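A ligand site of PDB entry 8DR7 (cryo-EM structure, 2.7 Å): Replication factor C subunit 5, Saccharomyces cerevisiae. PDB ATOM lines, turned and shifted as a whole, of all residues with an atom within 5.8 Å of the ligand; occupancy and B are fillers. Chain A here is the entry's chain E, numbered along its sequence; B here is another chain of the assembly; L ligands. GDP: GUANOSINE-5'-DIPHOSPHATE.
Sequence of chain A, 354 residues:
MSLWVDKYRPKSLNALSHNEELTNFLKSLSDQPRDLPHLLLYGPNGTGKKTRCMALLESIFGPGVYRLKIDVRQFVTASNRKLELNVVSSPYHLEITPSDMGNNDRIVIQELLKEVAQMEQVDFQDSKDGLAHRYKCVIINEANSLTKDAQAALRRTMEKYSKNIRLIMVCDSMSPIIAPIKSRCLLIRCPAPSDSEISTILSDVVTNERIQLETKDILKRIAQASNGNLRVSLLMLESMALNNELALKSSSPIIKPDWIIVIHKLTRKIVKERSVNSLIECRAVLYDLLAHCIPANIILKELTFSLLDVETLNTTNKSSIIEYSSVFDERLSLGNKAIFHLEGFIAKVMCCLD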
ATOM      1  N   TRP A   4     -20.641   5.863   0.591  1.00  0.00           N
ATOM      2  CA  TRP A   4     -19.803   6.664  -0.293  1.00  0.00           C
ATOM      3  C   TRP A   4     -18.332   6.537   0.071  1.00  0.00           C
ATOM      4  O   TRP A   4     -17.471   6.611  -0.818  1.00  0.00           O
ATOM      5  CB  TRP A   4     -20.228   8.130  -0.239  1.00  0.00           C
ATOM      6  CG  TRP A   4     -21.694   8.355  -0.483  1.00  0.00           C
ATOM      7  CD1 TRP A   4     -22.558   7.504  -1.115  1.00  0.00           C
ATOM      8  CD2 TRP A   4     -22.463   9.493  -0.090  1.00  0.00           C
ATOM      9  NE1 TRP A   4     -23.814   8.045  -1.141  1.00  0.00           N
ATOM     10  CE2 TRP A   4     -23.783   9.275  -0.522  1.00  0.00           C
ATOM     11  CE3 TRP A   4     -22.165  10.681   0.580  1.00  0.00           C
ATOM     12  CZ2 TRP A   4     -24.802  10.192  -0.305  1.00  0.00           C
ATOM     13  CZ3 TRP A   4     -23.184  11.598   0.797  1.00  0.00           C
ATOM     14  CH2 TRP A   4     -24.484  11.346   0.361  1.00  0.00           C
ATOM     15  N   VAL A   5     -18.021   6.341   1.347  1.00  0.00           N
ATOM     16  CA  VAL A   5     -16.625   6.201   1.764  1.00  0.00           C
ATOM     17  C   VAL A   5     -16.003   4.962   1.143  1.00  0.00           C
ATOM     18  O   VAL A   5     -14.783   4.902   0.931  1.00  0.00           O
ATOM     19  CB  VAL A   5     -16.526   6.162   3.298  1.00  0.00           C
ATOM     20  CG1 VAL A   5     -17.220   4.915   3.849  1.00  0.00           C
ATOM     21  CG2 VAL A   5     -15.074   6.217   3.746  1.00  0.00           C
ATOM     22  N   ASP A   6     -16.819   3.945   0.836  1.00  0.00           N
ATOM     23  CA  ASP A   6     -16.323   2.695   0.264  1.00  0.00           C
ATOM     24  C   ASP A   6     -16.518   2.612  -1.237  1.00  0.00           C
ATOM     25  O   ASP A   6     -15.738   1.932  -1.913  1.00  0.00           O
ATOM     26  CB  ASP A   6     -17.031   1.506   0.923  1.00  0.00           C
ATOM     27  CG  ASP A   6     -16.563   1.272   2.346  1.00  0.00           C
ATOM     28  OD1 ASP A   6     -15.694   2.029   2.831  1.00  0.00           O
ATOM     29  OD2 ASP A   6     -17.067   0.323   2.990  1.00  0.00           O
ATOM     30  N   TYR A   8     -16.254   4.997  -3.536  1.00  0.00           N
ATOM     31  CA  TYR A   8     -15.374   5.866  -4.290  1.00  0.00           C
ATOM     32  C   TYR A   8     -13.903   5.687  -3.909  1.00  0.00           C
ATOM     33  O   TYR A   8     -13.083   6.565  -4.182  1.00  0.00           O
ATOM     34  CB  TYR A   8     -15.783   7.329  -4.108  1.00  0.00           C
ATOM     35  CG  TYR A   8     -17.178   7.622  -4.613  1.00  0.00           C
ATOM     36  CD1 TYR A   8     -17.430   7.764  -5.972  1.00  0.00           C
ATOM     37  CD2 TYR A   8     -18.249   7.733  -3.729  1.00  0.00           C
ATOM     38  CE1 TYR A   8     -18.706   8.027  -6.428  1.00  0.00           C
ATOM     39  CE2 TYR A   8     -19.525   7.995  -4.185  1.00  0.00           C
ATOM     40  CZ  TYR A   8     -19.747   8.143  -5.539  1.00  0.00           C
ATOM     41  OH  TYR A   8     -21.020   8.399  -6.003  1.00  0.00           O
ATOM     42  N   ARG A   9     -13.559   4.568  -3.274  1.00  0.00           N
ATOM     43  CA  ARG A   9     -12.169   4.322  -2.917  1.00  0.00           C
ATOM     44  C   ARG A   9     -11.354   4.082  -4.174  1.00  0.00           C
ATOM     45  O   ARG A   9     -11.711   3.228  -4.993  1.00  0.00           O
ATOM     46  CB  ARG A   9     -12.070   3.114  -1.990  1.00  0.00           C
ATOM     47  CG  ARG A   9     -10.644   2.681  -1.681  1.00  0.00           C
ATOM     48  CD  ARG A   9     -10.546   1.981  -0.334  1.00  0.00           C
ATOM     49  NE  ARG A   9     -11.512   0.893  -0.226  1.00  0.00           N
ATOM     50  CZ  ARG A   9     -12.626   0.932   0.503  1.00  0.00           C
ATOM     51  NH1 ARG A   9     -12.967   1.998   1.196  1.00  0.00           N
ATOM     52  NH2 ARG A   9     -13.420  -0.136   0.527  1.00  0.00           N
ATOM     53  N   PRO A  10     -10.241   4.808  -4.376  1.00  0.00           N
ATOM     54  CA  PRO A  10      -9.431   4.576  -5.588  1.00  0.00           C
ATOM     55  C   PRO A  10      -8.828   3.178  -5.588  1.00  0.00           C
ATOM     56  O   PRO A  10      -8.525   2.604  -4.537  1.00  0.00           O
ATOM     57  CB  PRO A  10      -8.359   5.658  -5.496  1.00  0.00           C
ATOM     58  CG  PRO A  10      -8.278   6.010  -4.066  1.00  0.00           C
ATOM     59  CD  PRO A  10      -9.658   5.852  -3.523  1.00  0.00           C
ATOM     60  N   ALA A  15      -5.223   7.022  -9.525  1.00  0.00           N
ATOM     61  CA  ALA A  15      -6.496   7.561  -9.047  1.00  0.00           C
ATOM     62  C   ALA A  15      -6.358   8.304  -7.723  1.00  0.00           C
ATOM     63  O   ALA A  15      -7.361   8.828  -7.227  1.00  0.00           O
ATOM     64  CB  ALA A  15      -7.518   6.435  -8.912  1.00  0.00           C
ATOM     65  N   LEU A  16      -5.170   8.356  -7.141  1.00  0.00           N
ATOM     66  CA  LEU A  16      -4.975   9.064  -5.890  1.00  0.00           C
ATOM     67  C   LEU A  16      -5.128  10.565  -6.101  1.00  0.00           C
ATOM     68  O   LEU A  16      -4.772  11.107  -7.149  1.00  0.00           O
ATOM     69  CB  LEU A  16      -3.601   8.746  -5.305  1.00  0.00           C
ATOM     70  CG  LEU A  16      -3.334   7.279  -4.993  1.00  0.00           C
ATOM     71  CD1 LEU A  16      -1.930   7.085  -4.434  1.00  0.00           C
ATOM     72  CD2 LEU A  16      -4.368   6.721  -4.024  1.00  0.00           C
ATOM     73  N   SER A  17      -5.659  11.251  -5.086  1.00  0.00           N
ATOM     74  CA  SER A  17      -5.989  12.663  -5.185  1.00  0.00           C
ATOM     75  C   SER A  17      -5.271  13.531  -4.157  1.00  0.00           C
ATOM     76  O   SER A  17      -5.543  14.737  -4.107  1.00  0.00           O
ATOM     77  CB  SER A  17      -7.505  12.867  -5.039  1.00  0.00           C
ATOM     78  OG  SER A  17      -8.199  12.255  -6.110  1.00  0.00           O
ATOM     79  N   HIS A  18      -4.368  12.976  -3.361  1.00  0.00           N
ATOM     80  CA  HIS A  18      -3.639  13.771  -2.376  1.00  0.00           C
ATOM     81  C   HIS A  18      -2.277  13.142  -2.138  1.00  0.00           C
ATOM     82  O   HIS A  18      -2.064  11.954  -2.369  1.00  0.00           O
ATOM     83  CB  HIS A  18      -4.421  13.902  -1.059  1.00  0.00           C
ATOM     84  CG  HIS A  18      -4.640  12.603  -0.356  1.00  0.00           C
ATOM     85  ND1 HIS A  18      -3.776  12.126   0.617  1.00  0.00           N
ATOM     86  CD2 HIS A  18      -5.618  11.665  -0.471  1.00  0.00           C
ATOM     87  CE1 HIS A  18      -4.222  10.965   1.067  1.00  0.00           C
ATOM     88  NE2 HIS A  18      -5.331  10.663   0.423  1.00  0.00           N
ATOM     89  N   PRO A  44      -0.952   9.177  10.267  1.00  0.00           N
ATOM     90  CA  PRO A  44      -2.221   9.316  10.972  1.00  0.00           C
ATOM     91  C   PRO A  44      -3.281   8.363  10.443  1.00  0.00           C
ATOM     92  O   PRO A  44      -3.253   7.951   9.284  1.00  0.00           O
ATOM     93  CB  PRO A  44      -2.620  10.771  10.723  1.00  0.00           C
ATOM     94  CG  PRO A  44      -1.364  11.459  10.303  1.00  0.00           C
ATOM     95  CD  PRO A  44      -0.555  10.426   9.595  1.00  0.00           C
ATOM     96  N   ASN A  45      -4.214   8.000  11.322  1.00  0.00           N
ATOM     97  CA  ASN A  45      -5.286   7.084  10.946  1.00  0.00           C
ATOM     98  C   ASN A  45      -6.237   7.744   9.954  1.00  0.00           C
ATOM     99  O   ASN A  45      -6.476   8.950  10.002  1.00  0.00           O
ATOM    100  CB  ASN A  45      -6.061   6.634  12.187  1.00  0.00           C
ATOM    101  CG  ASN A  45      -5.375   5.520  12.938  1.00  0.00           C
ATOM    102  OD1 ASN A  45      -5.036   5.656  14.121  1.00  0.00           O
ATOM    103  ND2 ASN A  45      -5.164   4.397  12.265  1.00  0.00           N
ATOM    104  N   GLY A  46      -6.775   6.920   9.054  1.00  0.00           N
ATOM    105  CA  GLY A  46      -7.767   7.397   8.108  1.00  0.00           C
ATOM    106  C   GLY A  46      -7.228   8.290   7.013  1.00  0.00           C
ATOM    107  O   GLY A  46      -8.004   9.063   6.437  1.00  0.00           O
ATOM    108  N   THR A  47      -5.941   8.199   6.702  1.00  0.00           N
ATOM    109  CA  THR A  47      -5.349   9.015   5.648  1.00  0.00           C
ATOM    110  C   THR A  47      -5.255   8.297   4.309  1.00  0.00           C
ATOM    111  O   THR A  47      -5.171   8.980   3.274  1.00  0.00           O
ATOM    112  CB  THR A  47      -3.938   9.482   6.061  1.00  0.00           C
ATOM    113  OG1 THR A  47      -3.086   8.342   6.218  1.00  0.00           O
ATOM    114  CG2 THR A  47      -3.992  10.262   7.362  1.00  0.00           C
ATOM    115  N   GLY A  48      -5.263   6.971   4.297  1.00  0.00           N
ATOM    116  CA  GLY A  48      -5.225   6.221   3.047  1.00  0.00           C
ATOM    117  C   GLY A  48      -4.022   5.307   2.938  1.00  0.00           C
ATOM    118  O   GLY A  48      -3.608   4.972   1.822  1.00  0.00           O
ATOM    119  N   LYS A  49      -3.447   4.902   4.069  1.00  0.00           N
ATOM    120  CA  LYS A  49      -2.301   4.008   4.033  1.00  0.00           C
ATOM    121  C   LYS A  49      -2.665   2.656   3.424  1.00  0.00           C
ATOM    122  O   LYS A  49      -1.946   2.137   2.569  1.00  0.00           O
ATOM    123  CB  LYS A  49      -1.737   3.817   5.436  1.00  0.00           C
ATOM    124  CG  LYS A  49      -1.304   5.116   6.110  1.00  0.00           C
ATOM    125  CD  LYS A  49      -0.559   4.855   7.415  1.00  0.00           C
ATOM    126  CE  LYS A  49      -1.481   4.309   8.489  1.00  0.00           C
ATOM    127  NZ  LYS A  49      -2.635   5.206   8.775  1.00  0.00           N
ATOM    128  N   LYS A  50      -3.802   2.088   3.834  1.00  0.00           N
ATOM    129  CA  LYS A  50      -4.223   0.802   3.273  1.00  0.00           C
ATOM    130  C   LYS A  50      -4.574   0.939   1.807  1.00  0.00           C
ATOM    131  O   LYS A  50      -4.262   0.053   0.996  1.00  0.00           O
ATOM    132  CB  LYS A  50      -5.407   0.249   4.072  1.00  0.00           C
ATOM    133  CG  LYS A  50      -5.763  -1.193   3.767  1.00  0.00           C
ATOM    134  CD  LYS A  50      -4.657  -2.161   4.194  1.00  0.00           C
ATOM    135  CE  LYS A  50      -4.974  -3.595   3.815  1.00  0.00           C
ATOM    136  NZ  LYS A  50      -6.362  -3.987   4.189  1.00  0.00           N
ATOM    137  N   THR A  51      -5.242   2.039   1.434  1.00  0.00           N
ATOM    138  CA  THR A  51      -5.567   2.260   0.026  1.00  0.00           C
ATOM    139  C   THR A  51      -4.302   2.382  -0.816  1.00  0.00           C
ATOM    140  O   THR A  51      -4.232   1.833  -1.915  1.00  0.00           O
ATOM    141  CB  THR A  51      -6.438   3.506  -0.117  1.00  0.00           C
ATOM    142  OG1 THR A  51      -7.543   3.443   0.794  1.00  0.00           O
ATOM    143  CG2 THR A  51      -6.956   3.628  -1.542  1.00  0.00           C
ATOM    144  N   ARG A  52      -3.298   3.089  -0.300  1.00  0.00           N
ATOM    145  CA  ARG A  52      -2.039   3.225  -1.037  1.00  0.00           C
ATOM    146  C   ARG A  52      -1.321   1.886  -1.131  1.00  0.00           C
ATOM    147  O   ARG A  52      -0.710   1.579  -2.169  1.00  0.00           O
ATOM    148  CB  ARG A  52      -1.151   4.272  -0.372  1.00  0.00           C
ATOM    149  CG  ARG A  52      -1.313   5.664  -0.950  1.00  0.00           C
ATOM    150  CD  ARG A  52      -1.208   6.744   0.098  1.00  0.00           C
ATOM    151  NE  ARG A  52      -1.368   8.078  -0.471  1.00  0.00           N
ATOM    152  CZ  ARG A  52      -2.535   8.596  -0.824  1.00  0.00           C
ATOM    153  NH1 ARG A  52      -3.667   7.941  -0.674  1.00  0.00           N
ATOM    154  NH2 ARG A  52      -2.567   9.822  -1.357  1.00  0.00           N
ATOM    155  N   VAL A 170       1.393  -1.932   8.097  1.00  0.00           N
ATOM    156  CA  VAL A 170       0.759  -0.626   8.219  1.00  0.00           C
ATOM    157  C   VAL A 170       0.473  -0.385   9.693  1.00  0.00           C
ATOM    158  O   VAL A 170      -0.093  -1.245  10.378  1.00  0.00           O
ATOM    159  CB  VAL A 170      -0.529  -0.542   7.387  1.00  0.00           C
ATOM    160  CG1 VAL A 170      -1.087   0.873   7.414  1.00  0.00           C
ATOM    161  CG2 VAL A 170      -0.278  -1.004   5.964  1.00  0.00           C
ATOM    162  N   ILE A 201     -12.208  16.301  -2.540  1.00  0.00           N
ATOM    163  CA  ILE A 201     -12.747  14.942  -2.569  1.00  0.00           C
ATOM    164  C   ILE A 201     -14.225  14.957  -2.188  1.00  0.00           C
ATOM    165  O   ILE A 201     -15.054  14.283  -2.823  1.00  0.00           O
ATOM    166  CB  ILE A 201     -11.938  14.023  -1.648  1.00  0.00           C
ATOM    167  CG1 ILE A 201     -10.503  13.885  -2.168  1.00  0.00           C
ATOM    168  CG2 ILE A 201     -12.598  12.651  -1.557  1.00  0.00           C
ATOM    169  CD1 ILE A 201      -9.552  13.239  -1.174  1.00  0.00           C
ATOM    170  N   LEU A 230      -9.798  11.460   6.614  1.00  0.00           N
ATOM    171  CA  LEU A 230     -10.621  11.446   5.406  1.00  0.00           C
ATOM    172  C   LEU A 230     -11.826  10.511   5.525  1.00  0.00           C
ATOM    173  O   LEU A 230     -12.909  10.850   5.054  1.00  0.00           O
ATOM    174  CB  LEU A 230      -9.781  11.049   4.194  1.00  0.00           C
ATOM    175  CG  LEU A 230     -10.465  11.103   2.827  1.00  0.00           C
ATOM    176  CD1 LEU A 230     -11.183  12.433   2.607  1.00  0.00           C
ATOM    177  CD2 LEU A 230      -9.440  10.865   1.726  1.00  0.00           C
ATOM    178  N   ARG A 231     -11.637   9.335   6.133  1.00  0.00           N
ATOM    179  CA  ARG A 231     -12.772   8.442   6.360  1.00  0.00           C
ATOM    180  C   ARG A 231     -13.811   9.102   7.239  1.00  0.00           C
ATOM    181  O   ARG A 231     -15.023   9.003   6.969  1.00  0.00           O
ATOM    182  CB  ARG A 231     -12.277   7.135   6.984  1.00  0.00           C
ATOM    183  CG  ARG A 231     -13.401   6.205   7.432  1.00  0.00           C
ATOM    184  CD  ARG A 231     -12.856   4.876   7.943  1.00  0.00           C
ATOM    185  NE  ARG A 231     -11.852   5.057   8.989  1.00  0.00           N
ATOM    186  CZ  ARG A 231     -10.557   4.821   8.853  1.00  0.00           C
ATOM    187  NH1 ARG A 231     -10.044   4.395   7.710  1.00  0.00           N
ATOM    188  NH2 ARG A 231      -9.753   5.015   9.893  1.00  0.00           N
ATOM    189  N   LEU A 234     -15.721  11.660   5.121  1.00  0.00           N
ATOM    190  CA  LEU A 234     -16.705  11.059   4.230  1.00  0.00           C
ATOM    191  C   LEU A 234     -17.909  10.545   5.002  1.00  0.00           C
ATOM    192  O   LEU A 234     -19.060  10.744   4.571  1.00  0.00           O
ATOM    193  CB  LEU A 234     -16.058   9.930   3.418  1.00  0.00           C
ATOM    194  CG  LEU A 234     -15.115  10.388   2.302  1.00  0.00           C
ATOM    195  CD1 LEU A 234     -14.072   9.332   1.994  1.00  0.00           C
ATOM    196  CD2 LEU A 234     -15.906  10.743   1.053  1.00  0.00           C
ATOM    197  N   SER B 695     -12.866  -0.781   4.416  1.00  0.00           N
ATOM    198  CA  SER B 695     -11.408  -0.649   4.494  1.00  0.00           C
ATOM    199  C   SER B 695     -11.098   0.017   5.829  1.00  0.00           C
ATOM    200  O   SER B 695     -10.899   1.235   5.909  1.00  0.00           O
ATOM    201  CB  SER B 695     -10.866   0.155   3.314  1.00  0.00           C
ATOM    202  OG  SER B 695      -9.482   0.435   3.473  1.00  0.00           O
ATOM    203  N   THR B 696     -11.049  -0.787   6.886  1.00  0.00           N
ATOM    204  CA  THR B 696     -10.836  -0.300   8.245  1.00  0.00           C
ATOM    205  C   THR B 696     -10.736  -1.508   9.172  1.00  0.00           C
ATOM    206  O   THR B 696     -10.931  -2.654   8.753  1.00  0.00           O
ATOM    207  CB  THR B 696     -11.963   0.632   8.697  1.00  0.00           C
ATOM    208  OG1 THR B 696     -11.480   1.505   9.727  1.00  0.00           O
ATOM    209  CG2 THR B 696     -13.160  -0.164   9.225  1.00  0.00           C
ATOM    210  N   TYR B 705     -17.782   3.852  11.680  1.00  0.00           N
ATOM    211  CA  TYR B 705     -18.732   3.287  10.730  1.00  0.00           C
ATOM    212  C   TYR B 705     -20.110   3.076  11.343  1.00  0.00           C
ATOM    213  O   TYR B 705     -21.127   3.255  10.663  1.00  0.00           O
ATOM    214  CB  TYR B 705     -18.198   1.968  10.187  1.00  0.00           C
ATOM    215  CG  TYR B 705     -17.443   2.093   8.875  1.00  0.00           C
ATOM    216  CD1 TYR B 705     -18.123   2.132   7.668  1.00  0.00           C
ATOM    217  CD2 TYR B 705     -16.058   2.176   8.851  1.00  0.00           C
ATOM    218  CE1 TYR B 705     -17.434   2.250   6.475  1.00  0.00           C
ATOM    219  CE2 TYR B 705     -15.371   2.286   7.664  1.00  0.00           C
ATOM    220  CZ  TYR B 705     -16.059   2.330   6.477  1.00  0.00           C
ATOM    221  OH  TYR B 705     -15.372   2.440   5.290  1.00  0.00           O
HETATM  222  PB  GDP L   1      -5.896   4.177   6.846  1.00  0.00           P
HETATM  223  O1B GDP L   1      -5.124   5.153   7.694  1.00  0.00           O
HETATM  224  O2B GDP L   1      -6.948   3.500   7.695  1.00  0.00           O
HETATM  225  O3B GDP L   1      -4.955   3.145   6.273  1.00  0.00           O
HETATM  226  O3A GDP L   1      -6.640   4.992   5.617  1.00  0.00           O
HETATM  227  PA  GDP L   1      -7.834   4.353   4.679  1.00  0.00           P
HETATM  228  O1A GDP L   1      -7.226   3.432   3.641  1.00  0.00           O
HETATM  229  O2A GDP L   1      -8.783   3.563   5.546  1.00  0.00           O
HETATM  230  O5' GDP L   1      -8.637   5.578   3.919  1.00  0.00           O
HETATM  231  C5' GDP L   1      -9.965   5.841   4.289  1.00  0.00           C
HETATM  232  C4' GDP L   1     -10.788   6.290   3.085  1.00  0.00           C
HETATM  233  O4' GDP L   1     -10.201   7.679   2.503  1.00  0.00           O
HETATM  234  C3' GDP L   1     -10.721   5.432   2.107  1.00  0.00           C
HETATM  235  O3' GDP L   1     -11.795   4.398   2.256  1.00  0.00           O
HETATM  236  C2' GDP L   1     -10.973   6.280   0.857  1.00  0.00           C
HETATM  237  O2' GDP L   1     -12.298   6.395   0.616  1.00  0.00           O
HETATM  238  C1' GDP L   1     -10.378   7.669   1.200  1.00  0.00           C
HETATM  239  N9  GDP L   1      -9.070   7.844   0.540  1.00  0.00           N
HETATM  240  C8  GDP L   1      -7.851   7.467   0.953  1.00  0.00           C
HETATM  241  N7  GDP L   1      -6.975   7.863   0.003  1.00  0.00           N
HETATM  242  C5  GDP L   1      -7.658   8.457  -0.971  1.00  0.00           C
HETATM  243  C6  GDP L   1      -7.205   9.103  -2.289  1.00  0.00           C
HETATM  244  O6  GDP L   1      -6.057   9.113  -2.580  1.00  0.00           O
HETATM  245  N1  GDP L   1      -8.174   9.691  -3.159  1.00  0.00           N
HETATM  246  C2  GDP L   1      -9.561   9.685  -2.798  1.00  0.00           C
HETATM  247  N2  GDP L   1     -10.546  10.282  -3.681  1.00  0.00           N
HETATM  248  N3  GDP L   1      -9.991   9.067  -1.537  1.00  0.00           N
HETATM  249  C4  GDP L   1      -8.974   8.452  -0.629  1.00  0.00           C
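An oxygen (O3B) of the ligand is in hydrogen-bond range of the backbone NH (N) of Lys 50. The side-chain amino group (NZ) of Lys 49 is in salt-bridge range of an oxygen (O1B) of the ligand (2.7 Å). The guanidinium group (NH1) of Arg 231 lies within salt-bridge range of an oxygen (O2A) of the ligand (2.6 Å). A ring nitrogen (NE2) of His 18 is in hydrogen-bond range of a nitrogen (N7) of the ligand (3.3 Å). N of Thr 47 sits at hydrogen-bond distance from O1B of the ligand (3.3 Å). The guanidinium group (NH1) of Arg 9 is in hydrogen-bond range of an oxygen (O3') of the ligand. An oxygen (O6) of the ligand lies within hydrogen-bond range of the guanidinium group of Arg 52 (3.3 Å). The backbone NH (N) of Thr 51 lies within hydrogen-bond range of an oxygen (O1A) of the ligand (3.3 Å). An oxygen (O6) of the ligand lies within hydrogen-bond range of the backbone NH (N) of Ser 17 (3.3 Å). The backbone NH (N) of Gly 46 is in hydrogen-bond range of an oxygen (O1B) of the ligand. N of Gly 48 sits at hydrogen-bond distance from O3A of the ligand. N of Lys 49 sits at hydrogen-bond distance from O3B of the ligand, 3.2 Å away. O2' of the ligand sits at hydrogen-bond distance from O of Val 5 (2.9 Å). An oxygen (O1A) of the ligand sits at hydrogen-bond distance from the side-chain hydroxyl (OG1) of Thr 51 (2.9 Å).
The side-chain amino group (NZ) of Lys 49 is in hydrogen-bond range of the backbone carbonyl oxygen (O) of Pro 44. The backbone carbonyl oxygen (O) of Gly 46 is in hydrogen-bond range of the backbone NH (N) of Leu 230, 3.0 Å away. The side-chain carboxylate of Asp 6 is in salt-bridge range of the guanidinium group of Arg 9, at 3.2 Å. O of Pro 44 sits close to OG1 of Thr 47, at 3.1 Å. A ring nitrogen (NE2) of His 18 lies close to the backbone carbonyl oxygen (O) of Thr 47, at 3.3 Å. The guanidinium group of Arg 9 is in hydrogen-bond range of the backbone carbonyl oxygen of Val 5, at 3.4 Å. The backbone carbonyl oxygen of His 18 lies within hydrogen-bond range of the guanidinium group of Arg 52 (2.4 Å).
O2A of the ligand sits close to O of Ser 695 of chain B (3.2 Å). CG of Pro 10 touches C6 of the ligand, 3.7 Å away. CD2 of Leu 16 touches O6 of the ligand, at 3.3 Å. Pro 44 touches the ligand (O to O1B, 3.7 Å). Asn 45 touches the ligand (C to O1B, 3.6 Å). Ile 201 touches the ligand (CG2 to N2, 3.8 Å). Leu 230 touches the ligand. Leu 234 touches the ligand. Hydrophobic or aromatic side chains that line the ligand: Pro 10, Leu 16, His 18, Ile 201, Leu 230 and Leu 234. Within 4 Å of the ligand: Val 5, Arg 9, Pro 10, Leu 16, Ser 17, His 18, Pro 44, Asn 45, Gly 46, Thr 47, Gly 48, Lys 49, Lys 50, Thr 51, Arg 52, Ile 201, Leu 230, Arg 231, Leu 234 and Ser 695 of chain B.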
